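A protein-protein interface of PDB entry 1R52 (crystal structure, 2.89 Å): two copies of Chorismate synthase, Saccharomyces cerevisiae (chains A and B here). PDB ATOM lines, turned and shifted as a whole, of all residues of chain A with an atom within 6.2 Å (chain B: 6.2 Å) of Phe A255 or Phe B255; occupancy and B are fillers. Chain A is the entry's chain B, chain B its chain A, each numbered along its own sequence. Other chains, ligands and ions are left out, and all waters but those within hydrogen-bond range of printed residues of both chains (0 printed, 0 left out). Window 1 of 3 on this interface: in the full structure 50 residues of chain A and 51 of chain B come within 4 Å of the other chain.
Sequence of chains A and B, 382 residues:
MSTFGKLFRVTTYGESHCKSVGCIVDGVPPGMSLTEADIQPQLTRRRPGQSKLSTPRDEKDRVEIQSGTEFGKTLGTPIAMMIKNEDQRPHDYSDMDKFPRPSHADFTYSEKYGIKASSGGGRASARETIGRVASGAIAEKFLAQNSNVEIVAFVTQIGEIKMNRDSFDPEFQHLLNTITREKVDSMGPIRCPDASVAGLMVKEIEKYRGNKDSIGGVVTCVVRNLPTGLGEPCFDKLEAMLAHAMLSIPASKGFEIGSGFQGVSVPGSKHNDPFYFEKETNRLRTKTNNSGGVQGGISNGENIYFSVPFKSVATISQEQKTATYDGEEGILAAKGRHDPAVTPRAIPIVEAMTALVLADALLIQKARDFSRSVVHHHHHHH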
ATOM      1  N   GLU A 239     -14.555  34.623 -16.167  1.00  0.00           N
ATOM      2  CA  GLU A 239     -14.224  33.227 -15.851  1.00  0.00           C
ATOM      3  C   GLU A 239     -14.098  32.912 -14.373  1.00  0.00           C
ATOM      4  O   GLU A 239     -14.200  31.776 -13.984  1.00  0.00           O
ATOM      5  CB  GLU A 239     -12.903  32.788 -16.504  1.00  0.00           C
ATOM      6  CG  GLU A 239     -11.633  33.506 -16.090  1.00  0.00           C
ATOM      7  CD  GLU A 239     -11.330  34.715 -16.953  1.00  0.00           C
ATOM      8  OE1 GLU A 239     -12.257  35.529 -17.196  1.00  0.00           O
ATOM      9  OE2 GLU A 239     -10.162  34.869 -17.387  1.00  0.00           O
ATOM     10  N   ALA A 240     -13.814  33.910 -13.552  1.00  0.00           N
ATOM     11  CA  ALA A 240     -13.787  33.694 -12.122  1.00  0.00           C
ATOM     12  C   ALA A 240     -15.181  33.683 -11.581  1.00  0.00           C
ATOM     13  O   ALA A 240     -15.505  32.874 -10.687  1.00  0.00           O
ATOM     14  CB  ALA A 240     -12.993  34.702 -11.431  1.00  0.00           C
ATOM     15  N   LEU A 242     -17.767  32.750 -13.372  1.00  0.00           N
ATOM     16  CA  LEU A 242     -18.226  31.484 -13.844  1.00  0.00           C
ATOM     17  C   LEU A 242     -17.650  30.311 -13.059  1.00  0.00           C
ATOM     18  O   LEU A 242     -18.349  29.343 -12.753  1.00  0.00           O
ATOM     19  CB  LEU A 242     -17.856  31.320 -15.285  1.00  0.00           C
ATOM     20  CG  LEU A 242     -18.662  32.067 -16.338  1.00  0.00           C
ATOM     21  CD1 LEU A 242     -18.006  31.860 -17.731  1.00  0.00           C
ATOM     22  CD2 LEU A 242     -20.089  31.603 -16.416  1.00  0.00           C
ATOM     23  N   ALA A 243     -16.371  30.360 -12.728  1.00  0.00           N
ATOM     24  CA  ALA A 243     -15.775  29.291 -11.908  1.00  0.00           C
ATOM     25  C   ALA A 243     -16.414  29.216 -10.504  1.00  0.00           C
ATOM     26  O   ALA A 243     -16.688  28.117 -10.005  1.00  0.00           O
ATOM     27  CB  ALA A 243     -14.298  29.472 -11.795  1.00  0.00           C
ATOM     28  N   HIS A 244     -16.680  30.375  -9.903  1.00  0.00           N
ATOM     29  CA  HIS A 244     -17.319  30.426  -8.576  1.00  0.00           C
ATOM     30  C   HIS A 244     -18.705  29.790  -8.672  1.00  0.00           C
ATOM     31  O   HIS A 244     -19.183  29.101  -7.770  1.00  0.00           O
ATOM     32  CB  HIS A 244     -17.422  31.891  -8.088  1.00  0.00           C
ATOM     33  CG  HIS A 244     -18.264  32.089  -6.853  1.00  0.00           C
ATOM     34  ND1 HIS A 244     -19.605  32.400  -6.905  1.00  0.00           N
ATOM     35  CD2 HIS A 244     -17.958  32.030  -5.530  1.00  0.00           C
ATOM     36  CE1 HIS A 244     -20.091  32.491  -5.673  1.00  0.00           C
ATOM     37  NE2 HIS A 244     -19.115  32.264  -4.820  1.00  0.00           N
ATOM     38  N   MET A 246     -19.844  27.417 -10.920  1.00  0.00           N
ATOM     39  CA  MET A 246     -19.830  26.004 -11.208  1.00  0.00           C
ATOM     40  C   MET A 246     -19.357  25.215 -10.000  1.00  0.00           C
ATOM     41  O   MET A 246     -19.870  24.099  -9.723  1.00  0.00           O
ATOM     42  CB  MET A 246     -18.935  25.687 -12.380  1.00  0.00           C
ATOM     43  CG  MET A 246     -19.443  26.162 -13.770  1.00  0.00           C
ATOM     44  SD  MET A 246     -21.246  25.977 -14.135  1.00  0.00           S
ATOM     45  CE  MET A 246     -21.603  27.536 -14.637  1.00  0.00           C
ATOM     46  N   LEU A 247     -18.419  25.767  -9.235  1.00  0.00           N
ATOM     47  CA  LEU A 247     -17.869  24.992  -8.092  1.00  0.00           C
ATOM     48  C   LEU A 247     -18.786  24.857  -6.924  1.00  0.00           C
ATOM     49  O   LEU A 247     -18.658  23.910  -6.188  1.00  0.00           O
ATOM     50  CB  LEU A 247     -16.493  25.468  -7.651  1.00  0.00           C
ATOM     51  CG  LEU A 247     -15.618  24.402  -8.298  1.00  0.00           C
ATOM     52  CD1 LEU A 247     -14.692  24.966  -9.389  1.00  0.00           C
ATOM     53  CD2 LEU A 247     -14.914  23.626  -7.243  1.00  0.00           C
ATOM     54  N   LYS A 253     -16.269  19.091  -8.957  1.00  0.00           N
ATOM     55  CA  LYS A 253     -14.896  19.143  -8.453  1.00  0.00           C
ATOM     56  C   LYS A 253     -13.936  19.981  -9.277  1.00  0.00           C
ATOM     57  O   LYS A 253     -12.717  19.850  -9.153  1.00  0.00           O
ATOM     58  CB  LYS A 253     -14.298  17.779  -8.352  1.00  0.00           C
ATOM     59  CG  LYS A 253     -15.190  16.745  -7.804  1.00  0.00           C
ATOM     60  CD  LYS A 253     -15.476  16.929  -6.326  1.00  0.00           C
ATOM     61  CE  LYS A 253     -14.251  16.736  -5.371  1.00  0.00           C
ATOM     62  NZ  LYS A 253     -14.699  16.762  -3.895  1.00  0.00           N
ATOM     63  N   GLY A 254     -14.466  20.865 -10.104  1.00  0.00           N
ATOM     64  CA  GLY A 254     -13.592  21.792 -10.803  1.00  0.00           C
ATOM     65  C   GLY A 254     -14.213  22.600 -11.919  1.00  0.00           C
ATOM     66  O   GLY A 254     -15.372  22.655 -12.099  1.00  0.00           O
ATOM     67  N   PHE A 255     -13.389  23.215 -12.714  1.00  0.00           N
ATOM     68  CA  PHE A 255     -13.873  24.104 -13.768  1.00  0.00           C
ATOM     69  C   PHE A 255     -12.683  24.379 -14.679  1.00  0.00           C
ATOM     70  O   PHE A 255     -11.579  24.566 -14.189  1.00  0.00           O
ATOM     71  CB  PHE A 255     -14.430  25.409 -13.179  1.00  0.00           C
ATOM     72  CG  PHE A 255     -14.667  26.482 -14.196  1.00  0.00           C
ATOM     73  CD1 PHE A 255     -15.910  26.695 -14.740  1.00  0.00           C
ATOM     74  CD2 PHE A 255     -13.654  27.295 -14.570  1.00  0.00           C
ATOM     75  CE1 PHE A 255     -16.130  27.702 -15.649  1.00  0.00           C
ATOM     76  CE2 PHE A 255     -13.850  28.286 -15.517  1.00  0.00           C
ATOM     77  CZ  PHE A 255     -15.085  28.483 -16.064  1.00  0.00           C
ATOM     78  N   GLU A 256     -12.891  24.370 -15.979  1.00  0.00           N
ATOM     79  CA  GLU A 256     -11.828  24.809 -16.854  1.00  0.00           C
ATOM     80  C   GLU A 256     -12.454  25.526 -18.035  1.00  0.00           C
ATOM     81  O   GLU A 256     -13.535  25.175 -18.469  1.00  0.00           O
ATOM     82  CB  GLU A 256     -10.952  23.603 -17.332  1.00  0.00           C
ATOM     83  CG  GLU A 256     -11.709  22.573 -18.146  1.00  0.00           C
ATOM     84  CD  GLU A 256     -10.875  21.648 -18.989  1.00  0.00           C
ATOM     85  OE1 GLU A 256      -9.688  21.618 -18.856  1.00  0.00           O
ATOM     86  OE2 GLU A 256     -11.425  20.907 -19.819  1.00  0.00           O
ATOM     87  N   ILE A 257     -11.742  26.486 -18.598  1.00  0.00           N
ATOM     88  CA  ILE A 257     -12.282  27.241 -19.724  1.00  0.00           C
ATOM     89  C   ILE A 257     -11.322  27.267 -20.933  1.00  0.00           C
ATOM     90  O   ILE A 257     -10.115  27.408 -20.814  1.00  0.00           O
ATOM     91  CB  ILE A 257     -12.653  28.653 -19.284  1.00  0.00           C
ATOM     92  CG1 ILE A 257     -13.509  29.310 -20.372  1.00  0.00           C
ATOM     93  CG2 ILE A 257     -11.384  29.456 -18.941  1.00  0.00           C
ATOM     94  CD1 ILE A 257     -13.980  30.667 -20.007  1.00  0.00           C
ATOM     95  N   PHE A 261      -6.990  22.544 -19.235  1.00  0.00           N
ATOM     96  CA  PHE A 261      -5.926  21.666 -18.777  1.00  0.00           C
ATOM     97  C   PHE A 261      -5.112  21.000 -19.928  1.00  0.00           C
ATOM     98  O   PHE A 261      -3.926  20.955 -19.917  1.00  0.00           O
ATOM     99  CB  PHE A 261      -6.549  20.613 -17.868  1.00  0.00           C
ATOM    100  CG  PHE A 261      -6.633  21.031 -16.453  1.00  0.00           C
ATOM    101  CD1 PHE A 261      -5.510  21.076 -15.662  1.00  0.00           C
ATOM    102  CD2 PHE A 261      -7.824  21.370 -15.887  1.00  0.00           C
ATOM    103  CE1 PHE A 261      -5.592  21.462 -14.278  1.00  0.00           C
ATOM    104  CE2 PHE A 261      -7.924  21.765 -14.546  1.00  0.00           C
ATOM    105  CZ  PHE A 261      -6.808  21.827 -13.747  1.00  0.00           C
ATOM    106  N   PHE A 306     -16.672  25.988 -21.455  1.00  0.00           N
ATOM    107  CA  PHE A 306     -15.968  25.530 -20.288  1.00  0.00           C
ATOM    108  C   PHE A 306     -16.486  24.170 -19.876  1.00  0.00           C
ATOM    109  O   PHE A 306     -17.484  23.700 -20.363  1.00  0.00           O
ATOM    110  CB  PHE A 306     -16.162  26.524 -19.114  1.00  0.00           C
ATOM    111  CG  PHE A 306     -17.556  26.767 -18.761  1.00  0.00           C
ATOM    112  CD1 PHE A 306     -18.214  25.959 -17.911  1.00  0.00           C
ATOM    113  CD2 PHE A 306     -18.229  27.782 -19.313  1.00  0.00           C
ATOM    114  CE1 PHE A 306     -19.579  26.167 -17.638  1.00  0.00           C
ATOM    115  CE2 PHE A 306     -19.583  28.001 -19.012  1.00  0.00           C
ATOM    116  CZ  PHE A 306     -20.241  27.182 -18.206  1.00  0.00           C
ATOM    117  N   SER A 307     -15.815  23.519 -18.960  1.00  0.00           N
ATOM    118  CA  SER A 307     -16.207  22.174 -18.607  1.00  0.00           C
ATOM    119  C   SER A 307     -16.093  21.984 -17.105  1.00  0.00           C
ATOM    120  O   SER A 307     -15.164  22.517 -16.452  1.00  0.00           O
ATOM    121  CB  SER A 307     -15.320  21.146 -19.354  1.00  0.00           C
ATOM    122  OG  SER A 307     -15.702  21.016 -20.714  1.00  0.00           O
ATOM    123  N   VAL A 308     -16.991  21.158 -16.582  1.00  0.00           N
ATOM    124  CA  VAL A 308     -17.074  20.917 -15.167  1.00  0.00           C
ATOM    125  C   VAL A 308     -17.138  19.407 -14.870  1.00  0.00           C
ATOM    126  O   VAL A 308     -18.009  18.696 -15.305  1.00  0.00           O
ATOM    127  CB  VAL A 308     -18.334  21.615 -14.630  1.00  0.00           C
ATOM    128  CG1 VAL A 308     -18.423  21.511 -13.138  1.00  0.00           C
ATOM    129  CG2 VAL A 308     -18.350  23.070 -15.056  1.00  0.00           C
ATOM    130  N   PRO A 309     -16.223  18.898 -14.098  1.00  0.00           N
ATOM    131  CA  PRO A 309     -16.323  17.509 -13.688  1.00  0.00           C
ATOM    132  C   PRO A 309     -17.250  17.350 -12.548  1.00  0.00           C
ATOM    133  O   PRO A 309     -17.244  18.201 -11.681  1.00  0.00           O
ATOM    134  CB  PRO A 309     -14.929  17.212 -13.193  1.00  0.00           C
ATOM    135  CG  PRO A 309     -14.502  18.514 -12.592  1.00  0.00           C
ATOM    136  CD  PRO A 309     -15.022  19.545 -13.574  1.00  0.00           C
ATOM    137  N   GLU B 239     -14.544  25.752  -1.795  1.00  0.00           N
ATOM    138  CA  GLU B 239     -13.984  25.491  -3.130  1.00  0.00           C
ATOM    139  C   GLU B 239     -14.401  26.472  -4.216  1.00  0.00           C
ATOM    140  O   GLU B 239     -13.725  26.619  -5.227  1.00  0.00           O
ATOM    141  CB  GLU B 239     -14.358  24.093  -3.616  1.00  0.00           C
ATOM    142  CG  GLU B 239     -15.836  23.856  -3.825  1.00  0.00           C
ATOM    143  CD  GLU B 239     -16.457  23.206  -2.618  1.00  0.00           C
ATOM    144  OE1 GLU B 239     -16.277  23.765  -1.507  1.00  0.00           O
ATOM    145  OE2 GLU B 239     -17.081  22.131  -2.754  1.00  0.00           O
ATOM    146  N   ALA B 240     -15.544  27.099  -4.034  1.00  0.00           N
ATOM    147  CA  ALA B 240     -16.002  28.070  -4.999  1.00  0.00           C
ATOM    148  C   ALA B 240     -15.267  29.389  -4.770  1.00  0.00           C
ATOM    149  O   ALA B 240     -14.914  30.139  -5.731  1.00  0.00           O
ATOM    150  CB  ALA B 240     -17.466  28.236  -4.913  1.00  0.00           C
ATOM    151  N   LEU B 242     -12.271  29.497  -3.438  1.00  0.00           N
ATOM    152  CA  LEU B 242     -10.971  29.176  -3.957  1.00  0.00           C
ATOM    153  C   LEU B 242     -10.956  29.171  -5.486  1.00  0.00           C
ATOM    154  O   LEU B 242      -9.990  29.597  -6.090  1.00  0.00           O
ATOM    155  CB  LEU B 242     -10.546  27.815  -3.463  1.00  0.00           C
ATOM    156  CG  LEU B 242     -10.043  27.723  -2.038  1.00  0.00           C
ATOM    157  CD1 LEU B 242      -9.828  26.258  -1.707  1.00  0.00           C
ATOM    158  CD2 LEU B 242      -8.748  28.463  -1.802  1.00  0.00           C
ATOM    159  N   ALA B 243     -11.991  28.652  -6.130  1.00  0.00           N
ATOM    160  CA  ALA B 243     -12.009  28.644  -7.605  1.00  0.00           C
ATOM    161  C   ALA B 243     -12.048  30.058  -8.148  1.00  0.00           C
ATOM    162  O   ALA B 243     -11.356  30.392  -9.122  1.00  0.00           O
ATOM    163  CB  ALA B 243     -13.167  27.885  -8.143  1.00  0.00           C
ATOM    164  N   HIS B 244     -12.838  30.892  -7.491  1.00  0.00           N
ATOM    165  CA  HIS B 244     -12.987  32.289  -7.920  1.00  0.00           C
ATOM    166  C   HIS B 244     -11.607  32.959  -7.843  1.00  0.00           C
ATOM    167  O   HIS B 244     -11.239  33.790  -8.704  1.00  0.00           O
ATOM    168  CB  HIS B 244     -13.997  32.995  -7.014  1.00  0.00           C
ATOM    169  CG  HIS B 244     -14.071  34.470  -7.221  1.00  0.00           C
ATOM    170  ND1 HIS B 244     -13.357  35.353  -6.453  1.00  0.00           N
ATOM    171  CD2 HIS B 244     -14.780  35.225  -8.094  1.00  0.00           C
ATOM    172  CE1 HIS B 244     -13.564  36.588  -6.888  1.00  0.00           C
ATOM    173  NE2 HIS B 244     -14.437  36.543  -7.875  1.00  0.00           N
ATOM    174  N   MET B 246      -8.440  31.585  -7.909  1.00  0.00           N
ATOM    175  CA  MET B 246      -7.436  31.060  -8.815  1.00  0.00           C
ATOM    176  C   MET B 246      -7.724  31.495 -10.251  1.00  0.00           C
ATOM    177  O   MET B 246      -6.783  31.763 -11.010  1.00  0.00           O
ATOM    178  CB  MET B 246      -7.410  29.524  -8.783  1.00  0.00           C
ATOM    179  CG  MET B 246      -6.864  28.874  -7.494  1.00  0.00           C
ATOM    180  SD  MET B 246      -5.371  29.649  -6.746  1.00  0.00           S
ATOM    181  CE  MET B 246      -5.894  29.855  -5.150  1.00  0.00           C
ATOM    182  N   LEU B 247      -9.002  31.569 -10.648  1.00  0.00           N
ATOM    183  CA  LEU B 247      -9.315  31.904 -12.065  1.00  0.00           C
ATOM    184  C   LEU B 247      -9.121  33.338 -12.428  1.00  0.00           C
ATOM    185  O   LEU B 247      -8.948  33.630 -13.608  1.00  0.00           O
ATOM    186  CB  LEU B 247     -10.683  31.422 -12.533  1.00  0.00           C
ATOM    187  CG  LEU B 247     -10.343  30.127 -13.230  1.00  0.00           C
ATOM    188  CD1 LEU B 247     -10.916  28.913 -12.490  1.00  0.00           C
ATOM    189  CD2 LEU B 247     -10.689  30.229 -14.664  1.00  0.00           C
ATOM    190  N   LYS B 253      -6.346  28.989 -16.603  1.00  0.00           N
ATOM    191  CA  LYS B 253      -7.487  28.487 -17.367  1.00  0.00           C
ATOM    192  C   LYS B 253      -8.337  27.435 -16.659  1.00  0.00           C
ATOM    193  O   LYS B 253      -9.148  26.753 -17.289  1.00  0.00           O
ATOM    194  CB  LYS B 253      -7.057  27.865 -18.665  1.00  0.00           C
ATOM    195  CG  LYS B 253      -6.060  28.650 -19.455  1.00  0.00           C
ATOM    196  CD  LYS B 253      -6.543  29.981 -19.898  1.00  0.00           C
ATOM    197  CE  LYS B 253      -7.656  29.903 -20.931  1.00  0.00           C
ATOM    198  NZ  LYS B 253      -8.000  31.294 -21.459  1.00  0.00           N
ATOM    199  N   GLY B 254      -8.217  27.325 -15.346  1.00  0.00           N
ATOM    200  CA  GLY B 254      -9.142  26.483 -14.628  1.00  0.00           C
ATOM    201  C   GLY B 254      -8.760  26.234 -13.184  1.00  0.00           C
ATOM    202  O   GLY B 254      -7.942  26.901 -12.611  1.00  0.00           O
ATOM    203  N   PHE B 255      -9.351  25.212 -12.604  1.00  0.00           N
ATOM    204  CA  PHE B 255      -9.184  24.925 -11.200  1.00  0.00           C
ATOM    205  C   PHE B 255      -9.827  23.591 -10.983  1.00  0.00           C
ATOM    206  O   PHE B 255     -10.887  23.357 -11.517  1.00  0.00           O
ATOM    207  CB  PHE B 255      -9.927  25.973 -10.366  1.00  0.00           C
ATOM    208  CG  PHE B 255     -10.069  25.610  -8.920  1.00  0.00           C
ATOM    209  CD1 PHE B 255      -9.192  26.073  -7.992  1.00  0.00           C
ATOM    210  CD2 PHE B 255     -11.075  24.783  -8.504  1.00  0.00           C
ATOM    211  CE1 PHE B 255      -9.309  25.729  -6.657  1.00  0.00           C
ATOM    212  CE2 PHE B 255     -11.171  24.422  -7.149  1.00  0.00           C
ATOM    213  CZ  PHE B 255     -10.301  24.908  -6.243  1.00  0.00           C
ATOM    214  N   GLU B 256      -9.205  22.724 -10.210  1.00  0.00           N
ATOM    215  CA  GLU B 256      -9.851  21.485  -9.814  1.00  0.00           C
ATOM    216  C   GLU B 256      -9.380  21.122  -8.405  1.00  0.00           C
ATOM    217  O   GLU B 256      -8.228  21.379  -8.037  1.00  0.00           O
ATOM    218  CB  GLU B 256      -9.531  20.332 -10.803  1.00  0.00           C
ATOM    219  CG  GLU B 256      -8.051  20.115 -11.042  1.00  0.00           C
ATOM    220  CD  GLU B 256      -7.638  18.719 -11.445  1.00  0.00           C
ATOM    221  OE1 GLU B 256      -8.445  18.015 -11.947  1.00  0.00           O
ATOM    222  OE2 GLU B 256      -6.472  18.319 -11.282  1.00  0.00           O
ATOM    223  N   ILE B 257     -10.264  20.479  -7.654  1.00  0.00           N
ATOM    224  CA  ILE B 257      -9.991  20.114  -6.275  1.00  0.00           C
ATOM    225  C   ILE B 257     -10.155  18.598  -5.958  1.00  0.00           C
ATOM    226  O   ILE B 257     -11.045  17.904  -6.417  1.00  0.00           O
ATOM    227  CB  ILE B 257     -10.857  20.957  -5.352  1.00  0.00           C
ATOM    228  CG1 ILE B 257     -10.308  20.867  -3.933  1.00  0.00           C
ATOM    229  CG2 ILE B 257     -12.313  20.530  -5.435  1.00  0.00           C
ATOM    230  CD1 ILE B 257     -10.920  21.850  -3.012  1.00  0.00           C
ATOM    231  N   PHE B 261     -10.682  16.159 -12.141  1.00  0.00           N
ATOM    232  CA  PHE B 261     -11.061  15.668 -13.439  1.00  0.00           C
ATOM    233  C   PHE B 261     -10.717  14.168 -13.622  1.00  0.00           C
ATOM    234  O   PHE B 261     -11.487  13.427 -14.164  1.00  0.00           O
ATOM    235  CB  PHE B 261     -10.348  16.496 -14.485  1.00  0.00           C
ATOM    236  CG  PHE B 261     -11.067  17.717 -14.871  1.00  0.00           C
ATOM    237  CD1 PHE B 261     -12.167  17.654 -15.677  1.00  0.00           C
ATOM    238  CD2 PHE B 261     -10.643  18.939 -14.471  1.00  0.00           C
ATOM    239  CE1 PHE B 261     -12.844  18.806 -16.058  1.00  0.00           C
ATOM    240  CE2 PHE B 261     -11.305  20.080 -14.848  1.00  0.00           C
ATOM    241  CZ  PHE B 261     -12.411  20.005 -15.626  1.00  0.00           C
ATOM    242  N   PHE B 306      -5.553  21.380  -4.546  1.00  0.00           N
ATOM    243  CA  PHE B 306      -6.217  21.724  -5.792  1.00  0.00           C
ATOM    244  C   PHE B 306      -5.155  22.079  -6.818  1.00  0.00           C
ATOM    245  O   PHE B 306      -3.997  22.243  -6.490  1.00  0.00           O
ATOM    246  CB  PHE B 306      -7.186  22.906  -5.603  1.00  0.00           C
ATOM    247  CG  PHE B 306      -6.543  24.112  -5.057  1.00  0.00           C
ATOM    248  CD1 PHE B 306      -5.922  25.007  -5.868  1.00  0.00           C
ATOM    249  CD2 PHE B 306      -6.491  24.317  -3.718  1.00  0.00           C
ATOM    250  CE1 PHE B 306      -5.270  26.110  -5.347  1.00  0.00           C
ATOM    251  CE2 PHE B 306      -5.837  25.443  -3.188  1.00  0.00           C
ATOM    252  CZ  PHE B 306      -5.206  26.313  -4.016  1.00  0.00           C
ATOM    253  N   SER B 307      -5.553  22.181  -8.073  1.00  0.00           N
ATOM    254  CA  SER B 307      -4.588  22.417  -9.118  1.00  0.00           C
ATOM    255  C   SER B 307      -5.149  23.428 -10.100  1.00  0.00           C
ATOM    256  O   SER B 307      -6.340  23.419 -10.370  1.00  0.00           O
ATOM    257  CB  SER B 307      -4.254  21.065  -9.818  1.00  0.00           C
ATOM    258  OG  SER B 307      -3.311  20.325  -9.046  1.00  0.00           O
ATOM    259  N   VAL B 308      -4.264  24.236 -10.668  1.00  0.00           N
ATOM    260  CA  VAL B 308      -4.622  25.292 -11.584  1.00  0.00           C
ATOM    261  C   VAL B 308      -3.736  25.261 -12.840  1.00  0.00           C
ATOM    262  O   VAL B 308      -2.520  25.361 -12.749  1.00  0.00           O
ATOM    263  CB  VAL B 308      -4.395  26.608 -10.861  1.00  0.00           C
ATOM    264  CG1 VAL B 308      -4.866  27.782 -11.661  1.00  0.00           C
ATOM    265  CG2 VAL B 308      -5.069  26.569  -9.544  1.00  0.00           C
ATOM    266  N   PRO B 309      -4.303  25.150 -14.016  1.00  0.00           N
ATOM    267  CA  PRO B 309      -3.500  25.220 -15.229  1.00  0.00           C
ATOM    268  C   PRO B 309      -3.217  26.628 -15.598  1.00  0.00           C
ATOM    269  O   PRO B 309      -4.114  27.433 -15.482  1.00  0.00           O
ATOM    270  CB  PRO B 309      -4.415  24.625 -16.307  1.00  0.00           C
ATOM    271  CG  PRO B 309      -5.762  25.044 -15.881  1.00  0.00           C
ATOM    272  CD  PRO B 309      -5.711  24.936 -14.321  1.00  0.00           C
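Phe A255 touches just these residues of chain B: Leu B247 (3.8 Å), Gly B254 (3.1 Å) and Phe B255 (2.8 Å).
Of the printed residues of chain B, Phe A261 touches Glu B256 (3.4 Å), Phe B261 (3.8 Å), Ser B307 (3.8 Å) and Pro B309 (3.3 Å).
Of the printed residues of chain B, Ser A307 touches Phe B261 (3.8 Å).
Printed residues of chain A within 4 Å of Ala B243: Ala A243 (3.99 Å) and Leu A247 (3.5 Å).
Of the printed residues of chain A, Phe B255 touches Leu A247 (3.7 Å), Gly A254 (3.2 Å) and Phe A255 (2.8 Å).
Of the printed residues of chain A, Glu B256 touches Lys A253 (3.4 Å), Gly A254 (3.9 Å) and Phe A261 (3.4 Å).
The nearest residue of chain B that does not touch Phe A255 is Phe B261 (4.3 Å).
The nearest residue of chain A that does not touch Phe B255 is Phe A261 (4.2 Å).
The backbone carbonyl oxygen (O) of Lys B253 sits at hydrogen-bond distance from the backbone NH (N) of Ile A257, at 2.9 Å.
The backbone NH of Ile B257 is in hydrogen-bond range of the backbone carbonyl oxygen of Lys A253 (2.9 Å).
The backbone carbonyl oxygen of Phe B255 sits at hydrogen-bond distance from the backbone NH of Phe A255.
The side-chain carboxylate (OE1) of Glu B256 lies within hydrogen-bond range of the backbone NH (N) of Phe B261 (2.9 Å).
The backbone NH (N) of Lys B253 is in hydrogen-bond range of the backbone carbonyl oxygen (O) of Pro B309, at 2.9 Å.
The backbone NH of Ser B307 is in hydrogen-bond range of the backbone carbonyl oxygen of Glu B256 (2.8 Å).
The backbone carbonyl oxygen (O) of Glu A256 sits at hydrogen-bond distance from the backbone NH (N) of Ser A307 (2.9 Å).
The side-chain carboxylate of Glu A256 is in hydrogen-bond range of the backbone NH of Phe A261 (2.9 Å).
N of Lys A253 is in hydrogen-bond range of O of Pro A309.
Among the printed residues, merely in contact across the chains: Phe A255 with Gly B254, Gly A254 with Phe B255, Glu A256 with Lys B253, Phe A261 with Pro B309, Pro A309 with Phe B261, Lys A253 with Glu B256, Ala A240 with His B244, Phe A261 with Glu B256, His A244 with Ala B240, Ala A243 with Leu B247, Leu A247 with Ala B243, Leu A247 with Glu B239, Glu A239 with Leu B247, Glu A256 with Phe B261, Leu A247 with Phe B255, Leu A247 with Ala B240, His A244 with His B244, Phe A261 with Ser B307, Phe A261 with Phe B261, Phe A255 with Leu B247, Ser A307 with Phe B261, Ala A240 with Leu B247, Glu A256 with Gly B254, Gly A254 with Glu B256 and Ala A243 with Ala B243.
Of the 17 printed residues of chain A, 13 touch a printed residue of chain B.
Printed residues of chain A that touch a printed residue of chain B: Glu A239, Ala A240, Ala A243, His A244, Leu A247, Lys A253, Gly A254, Phe A255, Glu A256, Ile A257, Phe A261, Ser A307 and Pro A309.
Hydrophobic or aromatic side chains of chain A that line the printed part of chain B: Ala A240, Ala A243, His A244, Leu A247, Phe A255, Ile A257, Phe A261 and Pro A309.
Along chain A the printed residues that touch a printed residue of chain B span positions 239 to 309.
Hydrophobic or aromatic side chains of chain B that line the printed part of chain A: Ala B240, Ala B243, His B244, Leu B247, Phe B255, Ile B257, Phe B261 and Pro B309.
Among the printed residues, no Asp or Glu carboxylate lies within 4 Å of a Lys or Arg side-chain nitrogen of the other chain.
Glu A239 touches Leu B247, and with the chains exchanged Leu A247 touches Glu B239.
Ala A240 touches His B244, and with the chains exchanged His A244 touches Ala B240.
Ala A240 touches Leu B247, and with the chains exchanged Leu A247 touches Ala B240.
Ala A243 touches Leu B247, and with the chains exchanged Leu A247 touches Ala B243.
Positions printed for both chains: 239, 240, 242, 243, 244, 246, 247, 253, 254, 255, 256, 257, 261, 306, 307, 308 and 309.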
